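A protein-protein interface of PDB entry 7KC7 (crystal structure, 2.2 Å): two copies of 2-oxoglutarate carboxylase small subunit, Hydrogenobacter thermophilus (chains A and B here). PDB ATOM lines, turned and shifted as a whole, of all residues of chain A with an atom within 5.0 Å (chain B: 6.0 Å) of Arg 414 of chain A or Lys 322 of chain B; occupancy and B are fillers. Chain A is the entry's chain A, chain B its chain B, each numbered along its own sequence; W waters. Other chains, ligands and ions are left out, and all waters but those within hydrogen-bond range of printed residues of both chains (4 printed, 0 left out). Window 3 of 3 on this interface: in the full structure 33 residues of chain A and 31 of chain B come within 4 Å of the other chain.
NH2 of Arg 414 of chain A is in salt-bridge range of OE1 of Glu 36 of chain B. NH2 of Arg 414 of chain A is in salt-bridge range of OD2 of Asp 319 of chain B (3.7 Å). The backbone carbonyl oxygen of Ser 417 of chain A sits at hydrogen-bond distance from the guanidinium group of Arg 32 of chain B (3.2 Å). The side-chain hydroxyl of Ser 417 of chain A is in hydrogen-bond range of the backbone NH of Glu 36 of chain B, 3.4 Å away.
The backbone carbonyl oxygen (O) of Phe 376 of chain A lies within hydrogen-bond range of the guanidinium group (NE) of Arg 414 of chain A, 3.2 Å away. The backbone carbonyl oxygen of Trp 404 of chain A is in hydrogen-bond range of the guanidinium group of Arg 414 of chain A, at 2.8 Å. The backbone carbonyl oxygen (O) of Asp 413 of chain A is in hydrogen-bond range of the side-chain hydroxyl (OG) of Ser 417 of chain A, at 2.8 Å. The guanidinium group (NH2) of Arg 29 of chain B is in salt-bridge range of the side-chain carboxylate (OE2) of Glu 313 of chain B (2.9 Å). The side-chain amino group of Lys 322 of chain B lies within salt-bridge range of the side-chain carboxylate of Glu 36 of chain B (2.8 Å). OD1 of Asp 319 of chain B lies within hydrogen-bond range of N of Lys 322 of chain B (3.0 Å).
Among the printed residues, merely in contact across the chains: Ala 418 of chain A with Arg 32 of chain B, Ile 378 of chain A with Arg 32 of chain B, Asp 413 of chain A with Glu 36 of chain B, Arg 414 of chain A with Lys 322 of chain B, Phe 376 of chain A with Glu 313 of chain B and Phe 376 of chain A with Asp 319 of chain B.
Printed residues of chain B within 4 Å of Ile 378 of chain A: Arg 32 (3.5 Å). Of the printed residues of chain B, Asp 413 of chain A touches Glu 36. Arg 414 of chain A touches three residues of chain B. Met 415 of chain A touches none of the printed residues of chain B. Of the printed residues of chain A, Glu 36 of chain B touches Asp 413, Arg 414 and Ser 417. Printed residues of chain A within 4 Å of Asp 319 of chain B: Phe 376 and Arg 414. Printed residues of chain A within 4 Å of Lys 322 of chain B: Arg 414 (3.7 Å). The nearest residue of chain B that does not touch Arg 414 of chain A is Arg 32 of chain B (5.1 Å).
Of the 17 printed residues of chain A, 6 touch a printed residue of chain B. Hydrophobic or aromatic side chains of chain A within 4 Å of the printed part of chain B: Phe 376 and Ile 378.
No position is printed for both chains.
Water W3 bridges OE2 of Glu 36 of chain B (2.6 Å) and O of Phe 376 of chain A (2.9 Å). Water W2 lies within hydrogen-bond range of the side-chain carboxylate (OE2) of Glu 36 of chain B (2.7 Å), the backbone carbonyl oxygen (O) of Arg 414 of chain A (2.7 Å), the guanidinium group (NH1) of Arg 32 of chain B (3.2 Å) and the backbone NH (N) of Ala 418 of chain A (3.4 Å). Water W1 bridges N of Phe 376 of chain A and NH1 of Arg 29 of chain B. Water W4 lies within hydrogen-bond range of the guanidinium group of Arg 414 of chain A (2.9 Å), the side-chain carboxylate of Asp 319 of chain B (2.9 Å) and the side-chain amino group of Lys 322 of chain B (3.1 Å).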
ATOM      1  N   PHE A 376     -18.767 -14.247  19.715  1.00  0.00           N
ATOM      2  CA  PHE A 376     -18.794 -15.184  20.831  1.00  0.00           C
ATOM      3  C   PHE A 376     -17.840 -14.706  21.919  1.00  0.00           C
ATOM      4  O   PHE A 376     -16.666 -14.444  21.650  1.00  0.00           O
ATOM      5  CB  PHE A 376     -18.393 -16.571  20.321  1.00  0.00           C
ATOM      6  CG  PHE A 376     -18.360 -17.651  21.384  1.00  0.00           C
ATOM      7  CD1 PHE A 376     -17.247 -17.804  22.203  1.00  0.00           C
ATOM      8  CD2 PHE A 376     -19.405 -18.538  21.525  1.00  0.00           C
ATOM      9  CE1 PHE A 376     -17.198 -18.814  23.179  1.00  0.00           C
ATOM     10  CE2 PHE A 376     -19.366 -19.549  22.481  1.00  0.00           C
ATOM     11  CZ  PHE A 376     -18.266 -19.693  23.300  1.00  0.00           C
ATOM     12  N   GLY A 377     -18.357 -14.558  23.139  1.00  0.00           N
ATOM     13  CA  GLY A 377     -17.525 -14.147  24.251  1.00  0.00           C
ATOM     14  C   GLY A 377     -17.077 -12.702  24.221  1.00  0.00           C
ATOM     15  O   GLY A 377     -16.074 -12.368  24.855  1.00  0.00           O
ATOM     16  N   ILE A 378     -17.774 -11.822  23.515  1.00  0.00           N
ATOM     17  CA  ILE A 378     -17.397 -10.419  23.486  1.00  0.00           C
ATOM     18  C   ILE A 378     -18.537  -9.549  24.000  1.00  0.00           C
ATOM     19  O   ILE A 378     -19.675  -9.622  23.507  1.00  0.00           O
ATOM     20  CB  ILE A 378     -16.963  -9.956  22.082  1.00  0.00           C
ATOM     21  CG1 ILE A 378     -15.687 -10.692  21.649  1.00  0.00           C
ATOM     22  CG2 ILE A 378     -16.782  -8.437  22.104  1.00  0.00           C
ATOM     23  CD1 ILE A 378     -15.400 -10.526  20.125  1.00  0.00           C
ATOM     24  N   VAL A 403     -13.990  -9.472  27.292  1.00  0.00           N
ATOM     25  CA  VAL A 403     -14.034 -10.788  26.659  1.00  0.00           C
ATOM     26  C   VAL A 403     -14.070 -11.848  27.739  1.00  0.00           C
ATOM     27  O   VAL A 403     -13.659 -11.623  28.874  1.00  0.00           O
ATOM     28  CB  VAL A 403     -12.862 -11.077  25.694  1.00  0.00           C
ATOM     29  CG1 VAL A 403     -12.784 -10.013  24.598  1.00  0.00           C
ATOM     30  CG2 VAL A 403     -11.568 -11.225  26.511  1.00  0.00           C
ATOM     31  N   TRP A 404     -14.589 -13.011  27.372  1.00  0.00           N
ATOM     32  CA  TRP A 404     -14.651 -14.163  28.246  1.00  0.00           C
ATOM     33  C   TRP A 404     -14.158 -15.379  27.501  1.00  0.00           C
ATOM     34  O   TRP A 404     -14.524 -15.608  26.339  1.00  0.00           O
ATOM     35  CB  TRP A 404     -16.094 -14.402  28.749  1.00  0.00           C
ATOM     36  CG  TRP A 404     -16.156 -15.603  29.575  1.00  0.00           C
ATOM     37  CD1 TRP A 404     -15.966 -15.689  30.943  1.00  0.00           C
ATOM     38  CD2 TRP A 404     -16.419 -16.946  29.126  1.00  0.00           C
ATOM     39  NE1 TRP A 404     -16.081 -16.997  31.352  1.00  0.00           N
ATOM     40  CE2 TRP A 404     -16.360 -17.787  30.266  1.00  0.00           C
ATOM     41  CE3 TRP A 404     -16.697 -17.516  27.880  1.00  0.00           C
ATOM     42  CZ2 TRP A 404     -16.543 -19.163  30.189  1.00  0.00           C
ATOM     43  CZ3 TRP A 404     -16.883 -18.895  27.808  1.00  0.00           C
ATOM     44  CH2 TRP A 404     -16.822 -19.694  28.954  1.00  0.00           C
ATOM     45  N   ALA A 405     -13.405 -16.219  28.184  1.00  0.00           N
ATOM     46  CA  ALA A 405     -13.036 -17.474  27.547  1.00  0.00           C
ATOM     47  C   ALA A 405     -12.814 -18.527  28.611  1.00  0.00           C
ATOM     48  O   ALA A 405     -12.475 -18.196  29.757  1.00  0.00           O
ATOM     49  CB  ALA A 405     -11.763 -17.327  26.700  1.00  0.00           C
ATOM     50  N   PRO A 406     -12.907 -19.813  28.239  1.00  0.00           N
ATOM     51  CA  PRO A 406     -12.725 -20.876  29.225  1.00  0.00           C
ATOM     52  C   PRO A 406     -11.307 -21.027  29.670  1.00  0.00           C
ATOM     53  O   PRO A 406     -11.072 -21.481  30.785  1.00  0.00           O
ATOM     54  CB  PRO A 406     -13.208 -22.130  28.481  1.00  0.00           C
ATOM     55  CG  PRO A 406     -13.911 -21.640  27.244  1.00  0.00           C
ATOM     56  CD  PRO A 406     -13.246 -20.361  26.904  1.00  0.00           C
ATOM     57  N   VAL A 410      -6.957 -18.364  25.477  1.00  0.00           N
ATOM     58  CA  VAL A 410      -8.010 -18.004  24.520  1.00  0.00           C
ATOM     59  C   VAL A 410      -8.593 -16.649  24.891  1.00  0.00           C
ATOM     60  O   VAL A 410      -8.933 -15.852  24.024  1.00  0.00           O
ATOM     61  CB  VAL A 410      -9.069 -19.125  24.477  1.00  0.00           C
ATOM     62  CG1 VAL A 410     -10.236 -18.850  23.501  1.00  0.00           C
ATOM     63  CG2 VAL A 410      -8.374 -20.418  24.139  1.00  0.00           C
ATOM     64  N   ALA A 411      -8.692 -16.340  26.192  1.00  0.00           N
ATOM     65  CA  ALA A 411      -9.168 -15.005  26.525  1.00  0.00           C
ATOM     66  C   ALA A 411      -8.248 -13.951  25.928  1.00  0.00           C
ATOM     67  O   ALA A 411      -8.713 -12.941  25.358  1.00  0.00           O
ATOM     68  CB  ALA A 411      -9.259 -14.834  28.037  1.00  0.00           C
ATOM     69  N   VAL A 412      -6.935 -14.178  26.032  1.00  0.00           N
ATOM     70  CA  VAL A 412      -5.972 -13.229  25.488  1.00  0.00           C
ATOM     71  C   VAL A 412      -6.130 -13.129  23.970  1.00  0.00           C
ATOM     72  O   VAL A 412      -6.222 -12.024  23.419  1.00  0.00           O
ATOM     73  CB  VAL A 412      -4.536 -13.615  25.893  1.00  0.00           C
ATOM     74  CG1 VAL A 412      -3.522 -12.751  25.116  1.00  0.00           C
ATOM     75  CG2 VAL A 412      -4.340 -13.518  27.405  1.00  0.00           C
ATOM     76  N   ASP A 413      -6.230 -14.282  23.286  1.00  0.00           N
ATOM     77  CA  ASP A 413      -6.385 -14.286  21.825  1.00  0.00           C
ATOM     78  C   ASP A 413      -7.688 -13.612  21.401  1.00  0.00           C
ATOM     79  O   ASP A 413      -7.725 -12.899  20.385  1.00  0.00           O
ATOM     80  CB  ASP A 413      -6.338 -15.718  21.271  1.00  0.00           C
ATOM     81  CG  ASP A 413      -4.973 -16.366  21.425  1.00  0.00           C
ATOM     82  OD1 ASP A 413      -3.937 -15.646  21.343  1.00  0.00           O
ATOM     83  OD2 ASP A 413      -4.953 -17.604  21.615  1.00  0.00           O
ATOM     84  N   ARG A 414      -8.781 -13.872  22.139  1.00  0.00           N
ATOM     85  CA  ARG A 414     -10.059 -13.236  21.842  1.00  0.00           C
ATOM     86  C   ARG A 414     -10.007 -11.709  21.991  1.00  0.00           C
ATOM     87  O   ARG A 414     -10.635 -10.979  21.201  1.00  0.00           O
ATOM     88  CB  ARG A 414     -11.125 -13.828  22.737  1.00  0.00           C
ATOM     89  CG  ARG A 414     -12.420 -13.179  22.534  1.00  0.00           C
ATOM     90  CD  ARG A 414     -13.476 -14.120  23.059  1.00  0.00           C
ATOM     91  NE  ARG A 414     -13.596 -15.273  22.155  1.00  0.00           N
ATOM     92  CZ  ARG A 414     -14.036 -16.488  22.494  1.00  0.00           C
ATOM     93  NH1 ARG A 414     -14.404 -16.764  23.755  1.00  0.00           N
ATOM     94  NH2 ARG A 414     -14.111 -17.437  21.551  1.00  0.00           N
ATOM     95  N   MET A 415      -9.317 -11.213  23.038  1.00  0.00           N
ATOM     96  CA  MET A 415      -9.159  -9.774  23.258  1.00  0.00           C
ATOM     97  C   MET A 415      -8.281  -9.144  22.171  1.00  0.00           C
ATOM     98  O   MET A 415      -8.602  -8.069  21.637  1.00  0.00           O
ATOM     99  CB  MET A 415      -8.521  -9.520  24.654  1.00  0.00           C
ATOM    100  CG  MET A 415      -8.230  -8.033  24.836  1.00  0.00           C
ATOM    101  SD  MET A 415      -9.705  -6.996  24.795  1.00  0.00           S
ATOM    102  CE  MET A 415     -10.451  -7.296  26.419  1.00  0.00           C
ATOM    103  N   ARG A 416      -7.145  -9.794  21.849  1.00  0.00           N
ATOM    104  CA  ARG A 416      -6.247  -9.282  20.807  1.00  0.00           C
ATOM    105  C   ARG A 416      -6.997  -9.181  19.488  1.00  0.00           C
ATOM    106  O   ARG A 416      -6.942  -8.156  18.799  1.00  0.00           O
ATOM    107  CB  ARG A 416      -5.023 -10.197  20.658  1.00  0.00           C
ATOM    108  CG  ARG A 416      -4.069  -9.793  19.485  1.00  0.00           C
ATOM    109  CD  ARG A 416      -3.109 -10.943  19.015  1.00  0.00           C
ATOM    110  NE  ARG A 416      -3.875 -11.990  18.355  1.00  0.00           N
ATOM    111  CZ  ARG A 416      -4.049 -13.237  18.806  1.00  0.00           C
ATOM    112  NH1 ARG A 416      -3.469 -13.661  19.924  1.00  0.00           N
ATOM    113  NH2 ARG A 416      -4.822 -14.092  18.126  1.00  0.00           N
ATOM    114  N   SER A 417      -7.708 -10.252  19.139  1.00  0.00           N
ATOM    115  CA  SER A 417      -8.468 -10.316  17.906  1.00  0.00           C
ATOM    116  C   SER A 417      -9.612  -9.314  17.922  1.00  0.00           C
ATOM    117  O   SER A 417      -9.979  -8.789  16.869  1.00  0.00           O
ATOM    118  CB  SER A 417      -9.014 -11.737  17.694  1.00  0.00           C
ATOM    119  OG  SER A 417      -8.007 -12.727  17.583  1.00  0.00           O
ATOM    120  N   ALA A 418     -10.223  -9.054  19.084  1.00  0.00           N
ATOM    121  CA  ALA A 418     -11.276  -8.042  19.115  1.00  0.00           C
ATOM    122  C   ALA A 418     -10.683  -6.654  18.940  1.00  0.00           C
ATOM    123  O   ALA A 418     -11.233  -5.807  18.216  1.00  0.00           O
ATOM    124  CB  ALA A 418     -12.088  -8.182  20.412  1.00  0.00           C
ATOM    125  N   LEU A 419      -9.589  -6.377  19.655  1.00  0.00           N
ATOM    126  CA  LEU A 419      -8.908  -5.096  19.519  1.00  0.00           C
ATOM    127  C   LEU A 419      -8.453  -4.866  18.078  1.00  0.00           C
ATOM    128  O   LEU A 419      -8.555  -3.742  17.558  1.00  0.00           O
ATOM    129  CB  LEU A 419      -7.682  -5.050  20.437  1.00  0.00           C
ATOM    130  CG  LEU A 419      -7.892  -4.999  21.956  1.00  0.00           C
ATOM    131  CD1 LEU A 419      -6.651  -5.325  22.800  1.00  0.00           C
ATOM    132  CD2 LEU A 419      -8.442  -3.599  22.248  1.00  0.00           C
ATOM    133  N   ARG B  29     -17.761 -13.107  11.195  1.00  0.00           N
ATOM    134  CA  ARG B  29     -17.809 -14.193  12.186  1.00  0.00           C
ATOM    135  C   ARG B  29     -16.711 -15.214  11.907  1.00  0.00           C
ATOM    136  O   ARG B  29     -15.990 -15.634  12.816  1.00  0.00           O
ATOM    137  CB  ARG B  29     -19.188 -14.867  12.157  1.00  0.00           C
ATOM    138  CG  ARG B  29     -19.349 -16.132  12.966  1.00  0.00           C
ATOM    139  CD  ARG B  29     -19.532 -15.857  14.474  1.00  0.00           C
ATOM    140  NE  ARG B  29     -19.628 -17.105  15.201  1.00  0.00           N
ATOM    141  CZ  ARG B  29     -18.590 -17.757  15.729  1.00  0.00           C
ATOM    142  NH1 ARG B  29     -17.343 -17.269  15.638  1.00  0.00           N
ATOM    143  NH2 ARG B  29     -18.787 -18.917  16.337  1.00  0.00           N
ATOM    144  N   ARG B  32     -13.184 -13.769  12.565  1.00  0.00           N
ATOM    145  CA  ARG B  32     -12.874 -13.656  13.994  1.00  0.00           C
ATOM    146  C   ARG B  32     -12.453 -15.012  14.550  1.00  0.00           C
ATOM    147  O   ARG B  32     -11.418 -15.129  15.200  1.00  0.00           O
ATOM    148  CB  ARG B  32     -14.083 -13.094  14.760  1.00  0.00           C
ATOM    149  CG  ARG B  32     -13.863 -12.934  16.279  1.00  0.00           C
ATOM    150  CD  ARG B  32     -14.889 -12.017  16.986  1.00  0.00           C
ATOM    151  NE  ARG B  32     -15.057 -10.748  16.297  1.00  0.00           N
ATOM    152  CZ  ARG B  32     -14.104  -9.822  16.195  1.00  0.00           C
ATOM    153  NH1 ARG B  32     -12.888 -10.036  16.747  1.00  0.00           N
ATOM    154  NH2 ARG B  32     -14.359  -8.699  15.520  1.00  0.00           N
ATOM    155  N   ALA B  33     -13.217 -16.068  14.233  1.00  0.00           N
ATOM    156  CA  ALA B  33     -12.825 -17.407  14.660  1.00  0.00           C
ATOM    157  C   ALA B  33     -11.427 -17.737  14.181  1.00  0.00           C
ATOM    158  O   ALA B  33     -10.595 -18.210  14.967  1.00  0.00           O
ATOM    159  CB  ALA B  33     -13.824 -18.459  14.152  1.00  0.00           C
ATOM    160  N   GLU B  36      -8.731 -15.726  16.142  1.00  0.00           N
ATOM    161  CA  GLU B  36      -8.543 -16.279  17.483  1.00  0.00           C
ATOM    162  C   GLU B  36      -7.727 -17.571  17.439  1.00  0.00           C
ATOM    163  O   GLU B  36      -6.952 -17.858  18.375  1.00  0.00           O
ATOM    164  CB  GLU B  36      -9.906 -16.537  18.135  1.00  0.00           C
ATOM    165  CG  GLU B  36     -10.669 -15.260  18.485  1.00  0.00           C
ATOM    166  CD  GLU B  36     -12.034 -15.504  19.151  1.00  0.00           C
ATOM    167  OE1 GLU B  36     -12.422 -16.678  19.413  1.00  0.00           O
ATOM    168  OE2 GLU B  36     -12.757 -14.501  19.379  1.00  0.00           O
ATOM    169  N   LEU B  37      -7.890 -18.372  16.362  1.00  0.00           N
ATOM    170  CA  LEU B  37      -7.113 -19.592  16.213  1.00  0.00           C
ATOM    171  C   LEU B  37      -5.696 -19.326  15.735  1.00  0.00           C
ATOM    172  O   LEU B  37      -4.919 -20.276  15.595  1.00  0.00           O
ATOM    173  CB  LEU B  37      -7.776 -20.556  15.226  1.00  0.00           C
ATOM    174  CG  LEU B  37      -9.053 -21.237  15.697  1.00  0.00           C
ATOM    175  CD1 LEU B  37      -9.692 -21.997  14.571  1.00  0.00           C
ATOM    176  CD2 LEU B  37      -8.729 -22.177  16.891  1.00  0.00           C
ATOM    177  N   GLU B 313     -25.142 -21.276  20.618  1.00  0.00           N
ATOM    178  CA  GLU B 313     -23.875 -21.058  21.289  1.00  0.00           C
ATOM    179  C   GLU B 313     -24.043 -20.421  22.668  1.00  0.00           C
ATOM    180  O   GLU B 313     -23.207 -20.599  23.537  1.00  0.00           O
ATOM    181  CB  GLU B 313     -22.969 -20.159  20.436  1.00  0.00           C
ATOM    182  CG  GLU B 313     -22.649 -20.698  19.051  1.00  0.00           C
ATOM    183  CD  GLU B 313     -21.705 -19.840  18.229  1.00  0.00           C
ATOM    184  OE1 GLU B 313     -21.728 -18.587  18.379  1.00  0.00           O
ATOM    185  OE2 GLU B 313     -20.933 -20.441  17.433  1.00  0.00           O
ATOM    186  N   ASP B 319     -18.546 -23.001  20.692  1.00  0.00           N
ATOM    187  CA  ASP B 319     -18.230 -22.125  19.561  1.00  0.00           C
ATOM    188  C   ASP B 319     -18.329 -22.950  18.282  1.00  0.00           C
ATOM    189  O   ASP B 319     -17.392 -23.668  17.911  1.00  0.00           O
ATOM    190  CB  ASP B 319     -16.840 -21.513  19.740  1.00  0.00           C
ATOM    191  CG  ASP B 319     -16.481 -20.495  18.674  1.00  0.00           C
ATOM    192  OD1 ASP B 319     -17.043 -20.574  17.554  1.00  0.00           O
ATOM    193  OD2 ASP B 319     -15.630 -19.580  18.964  1.00  0.00           O
ATOM    194  N   ILE B 320     -19.475 -22.865  17.607  1.00  0.00           N
ATOM    195  CA  ILE B 320     -19.720 -23.791  16.507  1.00  0.00           C
ATOM    196  C   ILE B 320     -18.776 -23.506  15.354  1.00  0.00           C
ATOM    197  O   ILE B 320     -18.170 -24.427  14.783  1.00  0.00           O
ATOM    198  CB  ILE B 320     -21.182 -23.714  16.066  1.00  0.00           C
ATOM    199  CG1 ILE B 320     -22.036 -24.172  17.224  1.00  0.00           C
ATOM    200  CG2 ILE B 320     -21.382 -24.552  14.813  1.00  0.00           C
ATOM    201  CD1 ILE B 320     -23.469 -23.867  17.030  1.00  0.00           C
ATOM    202  N   VAL B 321     -18.621 -22.227  15.002  1.00  0.00           N
ATOM    203  CA  VAL B 321     -17.816 -21.882  13.841  1.00  0.00           C
ATOM    204  C   VAL B 321     -16.370 -22.290  14.060  1.00  0.00           C
ATOM    205  O   VAL B 321     -15.713 -22.849  13.158  1.00  0.00           O
ATOM    206  CB  VAL B 321     -17.928 -20.374  13.535  1.00  0.00           C
ATOM    207  CG1 VAL B 321     -17.011 -20.019  12.357  1.00  0.00           C
ATOM    208  CG2 VAL B 321     -19.378 -20.013  13.192  1.00  0.00           C
ATOM    209  N   LYS B 322     -15.851 -22.031  15.261  1.00  0.00           N
ATOM    210  CA  LYS B 322     -14.480 -22.422  15.562  1.00  0.00           C
ATOM    211  C   LYS B 322     -14.329 -23.935  15.509  1.00  0.00           C
ATOM    212  O   LYS B 322     -13.323 -24.448  15.002  1.00  0.00           O
ATOM    213  CB  LYS B 322     -14.050 -21.888  16.926  1.00  0.00           C
ATOM    214  CG  LYS B 322     -12.558 -21.969  17.139  1.00  0.00           C
ATOM    215  CD  LYS B 322     -12.124 -21.394  18.459  1.00  0.00           C
ATOM    216  CE  LYS B 322     -11.853 -19.915  18.348  1.00  0.00           C
ATOM    217  NZ  LYS B 322     -11.551 -19.354  19.684  1.00  0.00           N
ATOM    218  N   TRP B 323     -15.354 -24.668  15.966  1.00  0.00           N
ATOM    219  CA  TRP B 323     -15.295 -26.127  15.862  1.00  0.00           C
ATOM    220  C   TRP B 323     -15.305 -26.574  14.399  1.00  0.00           C
ATOM    221  O   TRP B 323     -14.595 -27.509  14.044  1.00  0.00           O
ATOM    222  CB  TRP B 323     -16.424 -26.814  16.674  1.00  0.00           C
ATOM    223  CG  TRP B 323     -15.915 -27.072  18.101  1.00  0.00           C
ATOM    224  CD1 TRP B 323     -16.345 -26.452  19.259  1.00  0.00           C
ATOM    225  CD2 TRP B 323     -14.894 -27.992  18.509  1.00  0.00           C
ATOM    226  NE1 TRP B 323     -15.627 -26.907  20.343  1.00  0.00           N
ATOM    227  CE2 TRP B 323     -14.736 -27.855  19.919  1.00  0.00           C
ATOM    228  CE3 TRP B 323     -14.102 -28.921  17.836  1.00  0.00           C
ATOM    229  CZ2 TRP B 323     -13.825 -28.604  20.636  1.00  0.00           C
ATOM    230  CZ3 TRP B 323     -13.198 -29.659  18.555  1.00  0.00           C
ATOM    231  CH2 TRP B 323     -13.063 -29.497  19.945  1.00  0.00           C
ATOM    232  N   GLN B 324     -16.060 -25.911  13.530  1.00  0.00           N
ATOM    233  CA  GLN B 324     -15.980 -26.252  12.105  1.00  0.00           C
ATOM    234  C   GLN B 324     -14.526 -26.256  11.617  1.00  0.00           C
ATOM    235  O   GLN B 324     -14.056 -27.204  10.979  1.00  0.00           O
ATOM    236  CB  GLN B 324     -16.788 -25.253  11.286  1.00  0.00           C
ATOM    237  CG  GLN B 324     -18.307 -25.370  11.300  1.00  0.00           C
ATOM    238  CD  GLN B 324     -18.895 -24.254  10.411  1.00  0.00           C
ATOM    239  OE1 GLN B 324     -18.625 -23.068  10.659  1.00  0.00           O
ATOM    240  NE2 GLN B 324     -19.594 -24.623   9.329  1.00  0.00           N
ATOM    241  N   ILE B 325     -13.797 -25.195  11.925  1.00  0.00           N
ATOM    242  CA  ILE B 325     -12.433 -25.075  11.447  1.00  0.00           C
ATOM    243  C   ILE B 325     -11.562 -26.142  12.091  1.00  0.00           C
ATOM    244  O   ILE B 325     -10.764 -26.805  11.415  1.00  0.00           O
ATOM    245  CB  ILE B 325     -11.940 -23.645  11.721  1.00  0.00           C
ATOM    246  CG1 ILE B 325     -12.884 -22.651  11.053  1.00  0.00           C
ATOM    247  CG2 ILE B 325     -10.540 -23.435  11.202  1.00  0.00           C
ATOM    248  CD1 ILE B 325     -12.825 -21.232  11.625  1.00  0.00           C
ATOM    249  N   ARG B 326     -11.711 -26.337  13.399  1.00  0.00           N
ATOM    250  CA  ARG B 326     -10.940 -27.370  14.076  1.00  0.00           C
ATOM    251  C   ARG B 326     -11.243 -28.737  13.461  1.00  0.00           C
ATOM    252  O   ARG B 326     -10.339 -29.538  13.226  1.00  0.00           O
ATOM    253  CB  ARG B 326     -11.253 -27.336  15.577  1.00  0.00           C
ATOM    254  CG  ARG B 326     -10.536 -26.216  16.455  1.00  0.00           C
ATOM    255  CD  ARG B 326     -10.789 -26.540  17.967  1.00  0.00           C
ATOM    256  NE  ARG B 326     -10.165 -25.616  18.905  1.00  0.00           N
ATOM    257  N   ILE B 327     -12.521 -29.022  13.215  1.00  0.00           N
ATOM    258  CA  ILE B 327     -12.913 -30.302  12.643  1.00  0.00           C
ATOM    259  C   ILE B 327     -12.346 -30.489  11.265  1.00  0.00           C
ATOM    260  O   ILE B 327     -11.930 -31.596  10.917  1.00  0.00           O
ATOM    261  CB  ILE B 327     -14.446 -30.460  12.626  1.00  0.00           C
ATOM    262  CG1 ILE B 327     -14.920 -30.758  14.041  1.00  0.00           C
ATOM    263  CG2 ILE B 327     -14.883 -31.503  11.600  1.00  0.00           C
ATOM    264  CD1 ILE B 327     -16.365 -30.551  14.195  1.00  0.00           C
HETATM  265  O   HOH W   1     -17.400 -14.581  17.202  1.00  0.00           O
HETATM  266  O   HOH W   2     -12.040 -11.955  19.102  1.00  0.00           O
HETATM  267  O   HOH W   3     -15.371 -14.845  19.139  1.00  0.00           O
HETATM  268  O   HOH W   4     -14.033 -20.336  21.283  1.00  0.00           O
